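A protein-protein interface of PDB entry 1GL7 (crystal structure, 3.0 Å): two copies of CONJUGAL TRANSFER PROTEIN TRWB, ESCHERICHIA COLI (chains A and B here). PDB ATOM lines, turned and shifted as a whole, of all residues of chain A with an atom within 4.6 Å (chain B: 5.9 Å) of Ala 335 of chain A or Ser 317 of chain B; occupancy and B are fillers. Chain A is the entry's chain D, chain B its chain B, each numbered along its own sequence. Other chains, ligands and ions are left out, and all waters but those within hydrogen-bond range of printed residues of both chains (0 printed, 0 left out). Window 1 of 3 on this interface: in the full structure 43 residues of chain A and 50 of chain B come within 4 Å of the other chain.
The side-chain amide nitrogen of Gln 331 of chain A lies within hydrogen-bond range of the side-chain hydroxyl of Ser 319 of chain B (3.3 Å). The side-chain hydroxyl (OG) of Ser 319 of chain B is in hydrogen-bond range of the side-chain hydroxyl (OG1) of Thr 332 of chain A, at 2.7 Å. The side-chain hydroxyl of Ser 346 of chain B lies within hydrogen-bond range of the backbone carbonyl oxygen of Phe 337 of chain A, at 2.6 Å. O of Arg 334 of chain A sits at hydrogen-bond distance from OG1 of Thr 348 of chain B. The side-chain hydroxyl (OG1) of Thr 348 of chain B is in hydrogen-bond range of the backbone carbonyl oxygen (O) of Phe 337 of chain A (3.1 Å). OD1 of Asp 349 of chain B sits at hydrogen-bond distance from NE2 of Gln 331 of chain A (3.3 Å). The side-chain hydroxyl (OG1) of Thr 352 of chain B lies within hydrogen-bond range of the side-chain amide nitrogen (NE2) of Gln 331 of chain A (2.9 Å).
The backbone carbonyl oxygen (O) of Gln 316 of chain B lies close to the side-chain amide oxygen (OD1) of Asn 59 of chain B, 3.0 Å away. The side-chain hydroxyl (OG) of Ser 317 of chain B lies within hydrogen-bond range of the side-chain amide oxygen (OE1) of Gln 316 of chain B, at 3.4 Å. The side-chain amide oxygen of Gln 320 of chain B is in hydrogen-bond range of the backbone NH of Gln 316 of chain B, 3.0 Å away. OE1 of Gln 320 of chain B sits at hydrogen-bond distance from N of Ser 317 of chain B. The guanidinium group (NH2) of Arg 334 of chain B lies within hydrogen-bond range of the backbone carbonyl oxygen (O) of Thr 318 of chain B, 3.3 Å away. The side-chain hydroxyl (OG) of Ser 346 of chain B is in hydrogen-bond range of the side-chain hydroxyl (OG1) of Thr 348 of chain B, at 3.1 Å.
Among the printed residues, merely in contact across the chains: Gln 331 of chain A with Thr 318 of chain B (3.97 Å), Thr 332 of chain A with Gln 320 of chain B (3.7 Å), Ala 335 of chain A with Ser 317 of chain B (3.4 Å), Ala 335 of chain A with Ser 346 of chain B (3.4 Å), Ala 335 of chain A with Thr 348 of chain B (3.2 Å), Ala 335 of chain A with Asp 349 of chain B (3.3 Å) and Ser 336 of chain A with Gln 316 of chain B (3.7 Å).
Of chain B, only Ser 317 (3.4 Å), Ser 346 (3.4 Å), Thr 348 (3.2 Å) and Asp 349 (3.3 Å) come within 4 Å of Ala 335 of chain A. Ala 61 of chain B touches none of the printed residues of chain A. Of the printed residues of chain A, Ser 317 of chain B touches Ala 335 (3.4 Å). Printed residues of chain A within 4 Å of Ser 346 of chain B: Ala 335 (3.4 Å) and Phe 337 (2.6 Å). Printed residues of chain A within 4 Å of Asp 349 of chain B: Gln 331 (3.3 Å) and Ala 335 (3.3 Å). Of the printed residues of chain A, Thr 352 of chain B touches Gln 331 (2.9 Å). The nearest residue of chain B that does not touch Ala 335 of chain A is Gln 316 of chain B (4.5 Å). The nearest printed residue of chain A that does not touch Ser 317 of chain B is Thr 332 of chain A (4.01 Å).
Hydrophobic or aromatic side chains of chain A that line the printed part of chain B: Ala 335. Among the printed residues, 14 pairs touch across the chains. Among the printed residues, no Asp or Glu carboxylate lies within 4 Å of a Lys or Arg side-chain nitrogen of the other chain.
1 position is printed for both chains.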
ATOM      1  N   GLN A 331     -15.619   8.093 -20.343  1.00  0.00           N
ATOM      2  CA  GLN A 331     -14.342   8.568 -19.825  1.00  0.00           C
ATOM      3  C   GLN A 331     -13.875   9.730 -20.691  1.00  0.00           C
ATOM      4  O   GLN A 331     -13.677  10.849 -20.209  1.00  0.00           O
ATOM      5  CB  GLN A 331     -13.293   7.467 -19.889  1.00  0.00           C
ATOM      6  CG  GLN A 331     -11.988   7.840 -19.199  1.00  0.00           C
ATOM      7  CD  GLN A 331     -10.850   6.890 -19.539  1.00  0.00           C
ATOM      8  OE1 GLN A 331     -10.987   5.667 -19.425  1.00  0.00           O
ATOM      9  NE2 GLN A 331      -9.714   7.450 -19.959  1.00  0.00           N
ATOM     10  N   THR A 332     -13.699   9.441 -21.976  1.00  0.00           N
ATOM     11  CA  THR A 332     -13.259  10.435 -22.945  1.00  0.00           C
ATOM     12  C   THR A 332     -14.087  11.703 -22.791  1.00  0.00           C
ATOM     13  O   THR A 332     -13.567  12.813 -22.750  1.00  0.00           O
ATOM     14  CB  THR A 332     -13.450   9.919 -24.391  1.00  0.00           C
ATOM     15  OG1 THR A 332     -12.799   8.659 -24.539  1.00  0.00           O
ATOM     16  CG2 THR A 332     -12.863  10.892 -25.397  1.00  0.00           C
ATOM     17  N   LEU A 333     -15.392  11.514 -22.696  1.00  0.00           N
ATOM     18  CA  LEU A 333     -16.292  12.633 -22.583  1.00  0.00           C
ATOM     19  C   LEU A 333     -15.990  13.515 -21.385  1.00  0.00           C
ATOM     20  O   LEU A 333     -15.734  14.711 -21.542  1.00  0.00           O
ATOM     21  CB  LEU A 333     -17.734  12.129 -22.529  1.00  0.00           C
ATOM     22  CG  LEU A 333     -18.828  13.174 -22.807  1.00  0.00           C
ATOM     23  CD1 LEU A 333     -18.439  13.998 -24.026  1.00  0.00           C
ATOM     24  CD2 LEU A 333     -20.177  12.481 -23.039  1.00  0.00           C
ATOM     25  N   ARG A 334     -16.013  12.931 -20.192  1.00  0.00           N
ATOM     26  CA  ARG A 334     -15.732  13.696 -18.983  1.00  0.00           C
ATOM     27  C   ARG A 334     -14.345  14.331 -19.040  1.00  0.00           C
ATOM     28  O   ARG A 334     -14.149  15.488 -18.659  1.00  0.00           O
ATOM     29  CB  ARG A 334     -15.814  12.795 -17.759  1.00  0.00           C
ATOM     30  CG  ARG A 334     -17.215  12.459 -17.311  1.00  0.00           C
ATOM     31  CD  ARG A 334     -17.163  11.561 -16.080  1.00  0.00           C
ATOM     32  NE  ARG A 334     -16.796  10.192 -16.430  1.00  0.00           N
ATOM     33  CZ  ARG A 334     -17.651   9.169 -16.457  1.00  0.00           C
ATOM     34  NH1 ARG A 334     -17.226   7.961 -16.797  1.00  0.00           N
ATOM     35  NH2 ARG A 334     -18.927   9.345 -16.124  1.00  0.00           N
ATOM     36  N   ALA A 335     -13.388  13.557 -19.531  1.00  0.00           N
ATOM     37  CA  ALA A 335     -12.015  14.015 -19.644  1.00  0.00           C
ATOM     38  C   ALA A 335     -11.894  15.292 -20.475  1.00  0.00           C
ATOM     39  O   ALA A 335     -10.901  16.005 -20.376  1.00  0.00           O
ATOM     40  CB  ALA A 335     -11.165  12.913 -20.259  1.00  0.00           C
ATOM     41  N   SER A 336     -12.907  15.592 -21.275  1.00  0.00           N
ATOM     42  CA  SER A 336     -12.864  16.765 -22.129  1.00  0.00           C
ATOM     43  C   SER A 336     -13.168  18.081 -21.434  1.00  0.00           C
ATOM     44  O   SER A 336     -12.936  19.154 -22.006  1.00  0.00           O
ATOM     45  CB  SER A 336     -13.784  16.543 -23.319  1.00  0.00           C
ATOM     46  OG  SER A 336     -13.368  15.371 -24.005  1.00  0.00           O
ATOM     47  N   PHE A 337     -13.675  17.994 -20.202  1.00  0.00           N
ATOM     48  CA  PHE A 337     -13.953  19.180 -19.388  1.00  0.00           C
ATOM     49  C   PHE A 337     -12.721  19.388 -18.525  1.00  0.00           C
ATOM     50  O   PHE A 337     -12.372  18.535 -17.716  1.00  0.00           O
ATOM     51  CB  PHE A 337     -15.160  18.959 -18.491  1.00  0.00           C
ATOM     52  CG  PHE A 337     -16.430  18.821 -19.237  1.00  0.00           C
ATOM     53  CD1 PHE A 337     -16.668  17.690 -20.006  1.00  0.00           C
ATOM     54  CD2 PHE A 337     -17.389  19.826 -19.185  1.00  0.00           C
ATOM     55  CE1 PHE A 337     -17.845  17.551 -20.716  1.00  0.00           C
ATOM     56  CE2 PHE A 337     -18.573  19.705 -19.890  1.00  0.00           C
ATOM     57  CZ  PHE A 337     -18.802  18.557 -20.660  1.00  0.00           C
ATOM     58  N   ASN B  59       1.059  12.584 -26.106  1.00  0.00           N
ATOM     59  CA  ASN B  59      -0.203  12.548 -25.399  1.00  0.00           C
ATOM     60  C   ASN B  59      -0.358  13.793 -24.567  1.00  0.00           C
ATOM     61  O   ASN B  59       0.604  14.269 -23.963  1.00  0.00           O
ATOM     62  CB  ASN B  59      -0.242  11.337 -24.485  1.00  0.00           C
ATOM     63  CG  ASN B  59      -1.532  11.243 -23.709  1.00  0.00           C
ATOM     64  OD1 ASN B  59      -2.490  10.580 -24.129  1.00  0.00           O
ATOM     65  ND2 ASN B  59      -1.575  11.919 -22.568  1.00  0.00           N
ATOM     66  N   GLY B  60      -1.580  14.305 -24.520  1.00  0.00           N
ATOM     67  CA  GLY B  60      -1.853  15.497 -23.740  1.00  0.00           C
ATOM     68  C   GLY B  60      -3.271  15.959 -23.982  1.00  0.00           C
ATOM     69  O   GLY B  60      -3.870  15.620 -25.006  1.00  0.00           O
ATOM     70  N   ALA B  61      -3.815  16.726 -23.042  1.00  0.00           N
ATOM     71  CA  ALA B  61      -5.183  17.227 -23.167  1.00  0.00           C
ATOM     72  C   ALA B  61      -5.308  18.240 -24.295  1.00  0.00           C
ATOM     73  O   ALA B  61      -4.337  18.537 -25.002  1.00  0.00           O
ATOM     74  CB  ALA B  61      -5.645  17.854 -21.858  1.00  0.00           C
ATOM     75  N   LEU B 315      -2.571  11.802 -28.943  1.00  0.00           N
ATOM     76  CA  LEU B 315      -3.738  11.264 -28.240  1.00  0.00           C
ATOM     77  C   LEU B 315      -4.125  12.126 -27.060  1.00  0.00           C
ATOM     78  O   LEU B 315      -3.336  12.938 -26.586  1.00  0.00           O
ATOM     79  CB  LEU B 315      -3.490   9.856 -27.698  1.00  0.00           C
ATOM     80  CG  LEU B 315      -3.746   8.671 -28.622  1.00  0.00           C
ATOM     81  CD1 LEU B 315      -4.664   9.103 -29.799  1.00  0.00           C
ATOM     82  CD2 LEU B 315      -2.396   8.142 -29.114  1.00  0.00           C
ATOM     83  N   GLN B 316      -5.343  11.926 -26.579  1.00  0.00           N
ATOM     84  CA  GLN B 316      -5.832  12.666 -25.428  1.00  0.00           C
ATOM     85  C   GLN B 316      -6.071  11.664 -24.289  1.00  0.00           C
ATOM     86  O   GLN B 316      -5.253  11.565 -23.381  1.00  0.00           O
ATOM     87  CB  GLN B 316      -7.136  13.408 -25.768  1.00  0.00           C
ATOM     88  CG  GLN B 316      -7.485  14.520 -24.763  1.00  0.00           C
ATOM     89  CD  GLN B 316      -8.961  14.944 -24.759  1.00  0.00           C
ATOM     90  OE1 GLN B 316      -9.848  14.170 -24.369  1.00  0.00           O
ATOM     91  NE2 GLN B 316      -9.223  16.187 -25.180  1.00  0.00           N
ATOM     92  N   SER B 317      -7.185  10.927 -24.348  1.00  0.00           N
ATOM     93  CA  SER B 317      -7.539   9.920 -23.332  1.00  0.00           C
ATOM     94  C   SER B 317      -7.242   8.529 -23.882  1.00  0.00           C
ATOM     95  O   SER B 317      -7.406   8.288 -25.082  1.00  0.00           O
ATOM     96  CB  SER B 317      -9.025  10.017 -22.976  1.00  0.00           C
ATOM     97  OG  SER B 317      -9.371  11.346 -22.624  1.00  0.00           O
ATOM     98  N   THR B 318      -6.803   7.615 -23.022  1.00  0.00           N
ATOM     99  CA  THR B 318      -6.476   6.275 -23.502  1.00  0.00           C
ATOM    100  C   THR B 318      -7.726   5.550 -23.964  1.00  0.00           C
ATOM    101  O   THR B 318      -7.670   4.688 -24.837  1.00  0.00           O
ATOM    102  CB  THR B 318      -5.769   5.420 -22.421  1.00  0.00           C
ATOM    103  OG1 THR B 318      -6.566   5.388 -21.230  1.00  0.00           O
ATOM    104  CG2 THR B 318      -4.386   5.993 -22.102  1.00  0.00           C
ATOM    105  N   SER B 319      -8.856   5.930 -23.381  1.00  0.00           N
ATOM    106  CA  SER B 319     -10.134   5.327 -23.711  1.00  0.00           C
ATOM    107  C   SER B 319     -10.496   5.509 -25.177  1.00  0.00           C
ATOM    108  O   SER B 319     -11.227   4.702 -25.741  1.00  0.00           O
ATOM    109  CB  SER B 319     -11.215   5.941 -22.841  1.00  0.00           C
ATOM    110  OG  SER B 319     -11.132   7.353 -22.892  1.00  0.00           O
ATOM    111  N   GLN B 320      -9.986   6.570 -25.791  1.00  0.00           N
ATOM    112  CA  GLN B 320     -10.261   6.846 -27.198  1.00  0.00           C
ATOM    113  C   GLN B 320      -9.760   5.715 -28.088  1.00  0.00           C
ATOM    114  O   GLN B 320     -10.546   4.963 -28.655  1.00  0.00           O
ATOM    115  CB  GLN B 320      -9.565   8.126 -27.647  1.00  0.00           C
ATOM    116  CG  GLN B 320      -9.855   9.345 -26.824  1.00  0.00           C
ATOM    117  CD  GLN B 320      -9.091  10.534 -27.346  1.00  0.00           C
ATOM    118  OE1 GLN B 320      -7.855  10.531 -27.377  1.00  0.00           O
ATOM    119  NE2 GLN B 320      -9.816  11.556 -27.783  1.00  0.00           N
ATOM    120  N   LEU B 321      -8.441   5.615 -28.211  1.00  0.00           N
ATOM    121  CA  LEU B 321      -7.826   4.595 -29.040  1.00  0.00           C
ATOM    122  C   LEU B 321      -8.336   3.204 -28.692  1.00  0.00           C
ATOM    123  O   LEU B 321      -8.442   2.334 -29.560  1.00  0.00           O
ATOM    124  CB  LEU B 321      -6.308   4.623 -28.886  1.00  0.00           C
ATOM    125  CG  LEU B 321      -5.578   3.838 -29.979  1.00  0.00           C
ATOM    126  CD1 LEU B 321      -5.403   4.715 -31.234  1.00  0.00           C
ATOM    127  CD2 LEU B 321      -4.246   3.385 -29.444  1.00  0.00           C
ATOM    128  N   ARG B 334       0.087   1.374 -29.094  1.00  0.00           N
ATOM    129  CA  ARG B 334       0.806   2.398 -28.335  1.00  0.00           C
ATOM    130  C   ARG B 334       2.230   1.947 -28.057  1.00  0.00           C
ATOM    131  O   ARG B 334       3.198   2.689 -28.278  1.00  0.00           O
ATOM    132  CB  ARG B 334       0.092   2.682 -27.013  1.00  0.00           C
ATOM    133  CG  ARG B 334      -1.193   3.463 -27.164  1.00  0.00           C
ATOM    134  CD  ARG B 334      -1.782   3.795 -25.813  1.00  0.00           C
ATOM    135  NE  ARG B 334      -2.606   2.715 -25.301  1.00  0.00           N
ATOM    136  CZ  ARG B 334      -3.935   2.747 -25.264  1.00  0.00           C
ATOM    137  NH1 ARG B 334      -4.595   1.702 -24.784  1.00  0.00           N
ATOM    138  NH2 ARG B 334      -4.606   3.823 -25.686  1.00  0.00           N
ATOM    139  N   SER B 346      -6.572  16.789 -17.990  1.00  0.00           N
ATOM    140  CA  SER B 346      -7.627  17.283 -17.115  1.00  0.00           C
ATOM    141  C   SER B 346      -7.757  16.440 -15.871  1.00  0.00           C
ATOM    142  O   SER B 346      -7.457  15.252 -15.888  1.00  0.00           O
ATOM    143  CB  SER B 346      -8.966  17.282 -17.853  1.00  0.00           C
ATOM    144  OG  SER B 346     -10.013  17.761 -17.023  1.00  0.00           O
ATOM    145  N   THR B 348     -10.463  15.637 -14.527  1.00  0.00           N
ATOM    146  CA  THR B 348     -11.651  14.817 -14.674  1.00  0.00           C
ATOM    147  C   THR B 348     -11.346  13.449 -15.241  1.00  0.00           C
ATOM    148  O   THR B 348     -12.227  12.596 -15.291  1.00  0.00           O
ATOM    149  CB  THR B 348     -12.693  15.485 -15.581  1.00  0.00           C
ATOM    150  OG1 THR B 348     -12.170  15.588 -16.914  1.00  0.00           O
ATOM    151  CG2 THR B 348     -13.058  16.871 -15.055  1.00  0.00           C
ATOM    152  N   ASP B 349     -10.110  13.237 -15.684  1.00  0.00           N
ATOM    153  CA  ASP B 349      -9.738  11.939 -16.236  1.00  0.00           C
ATOM    154  C   ASP B 349      -8.593  11.310 -15.465  1.00  0.00           C
ATOM    155  O   ASP B 349      -7.502  11.111 -15.994  1.00  0.00           O
ATOM    156  CB  ASP B 349      -9.347  12.066 -17.698  1.00  0.00           C
ATOM    157  CG  ASP B 349      -8.940  10.742 -18.294  1.00  0.00           C
ATOM    158  OD1 ASP B 349      -9.119   9.705 -17.611  1.00  0.00           O
ATOM    159  OD2 ASP B 349      -8.450  10.737 -19.441  1.00  0.00           O
ATOM    160  N   THR B 352      -6.513   8.174 -17.069  1.00  0.00           N
ATOM    161  CA  THR B 352      -5.451   8.395 -18.031  1.00  0.00           C
ATOM    162  C   THR B 352      -4.228   9.025 -17.356  1.00  0.00           C
ATOM    163  O   THR B 352      -3.091   8.726 -17.725  1.00  0.00           O
ATOM    164  CB  THR B 352      -5.929   9.254 -19.212  1.00  0.00           C
ATOM    165  OG1 THR B 352      -7.059   8.625 -19.834  1.00  0.00           O
ATOM    166  CG2 THR B 352      -4.817   9.374 -20.252  1.00  0.00           C
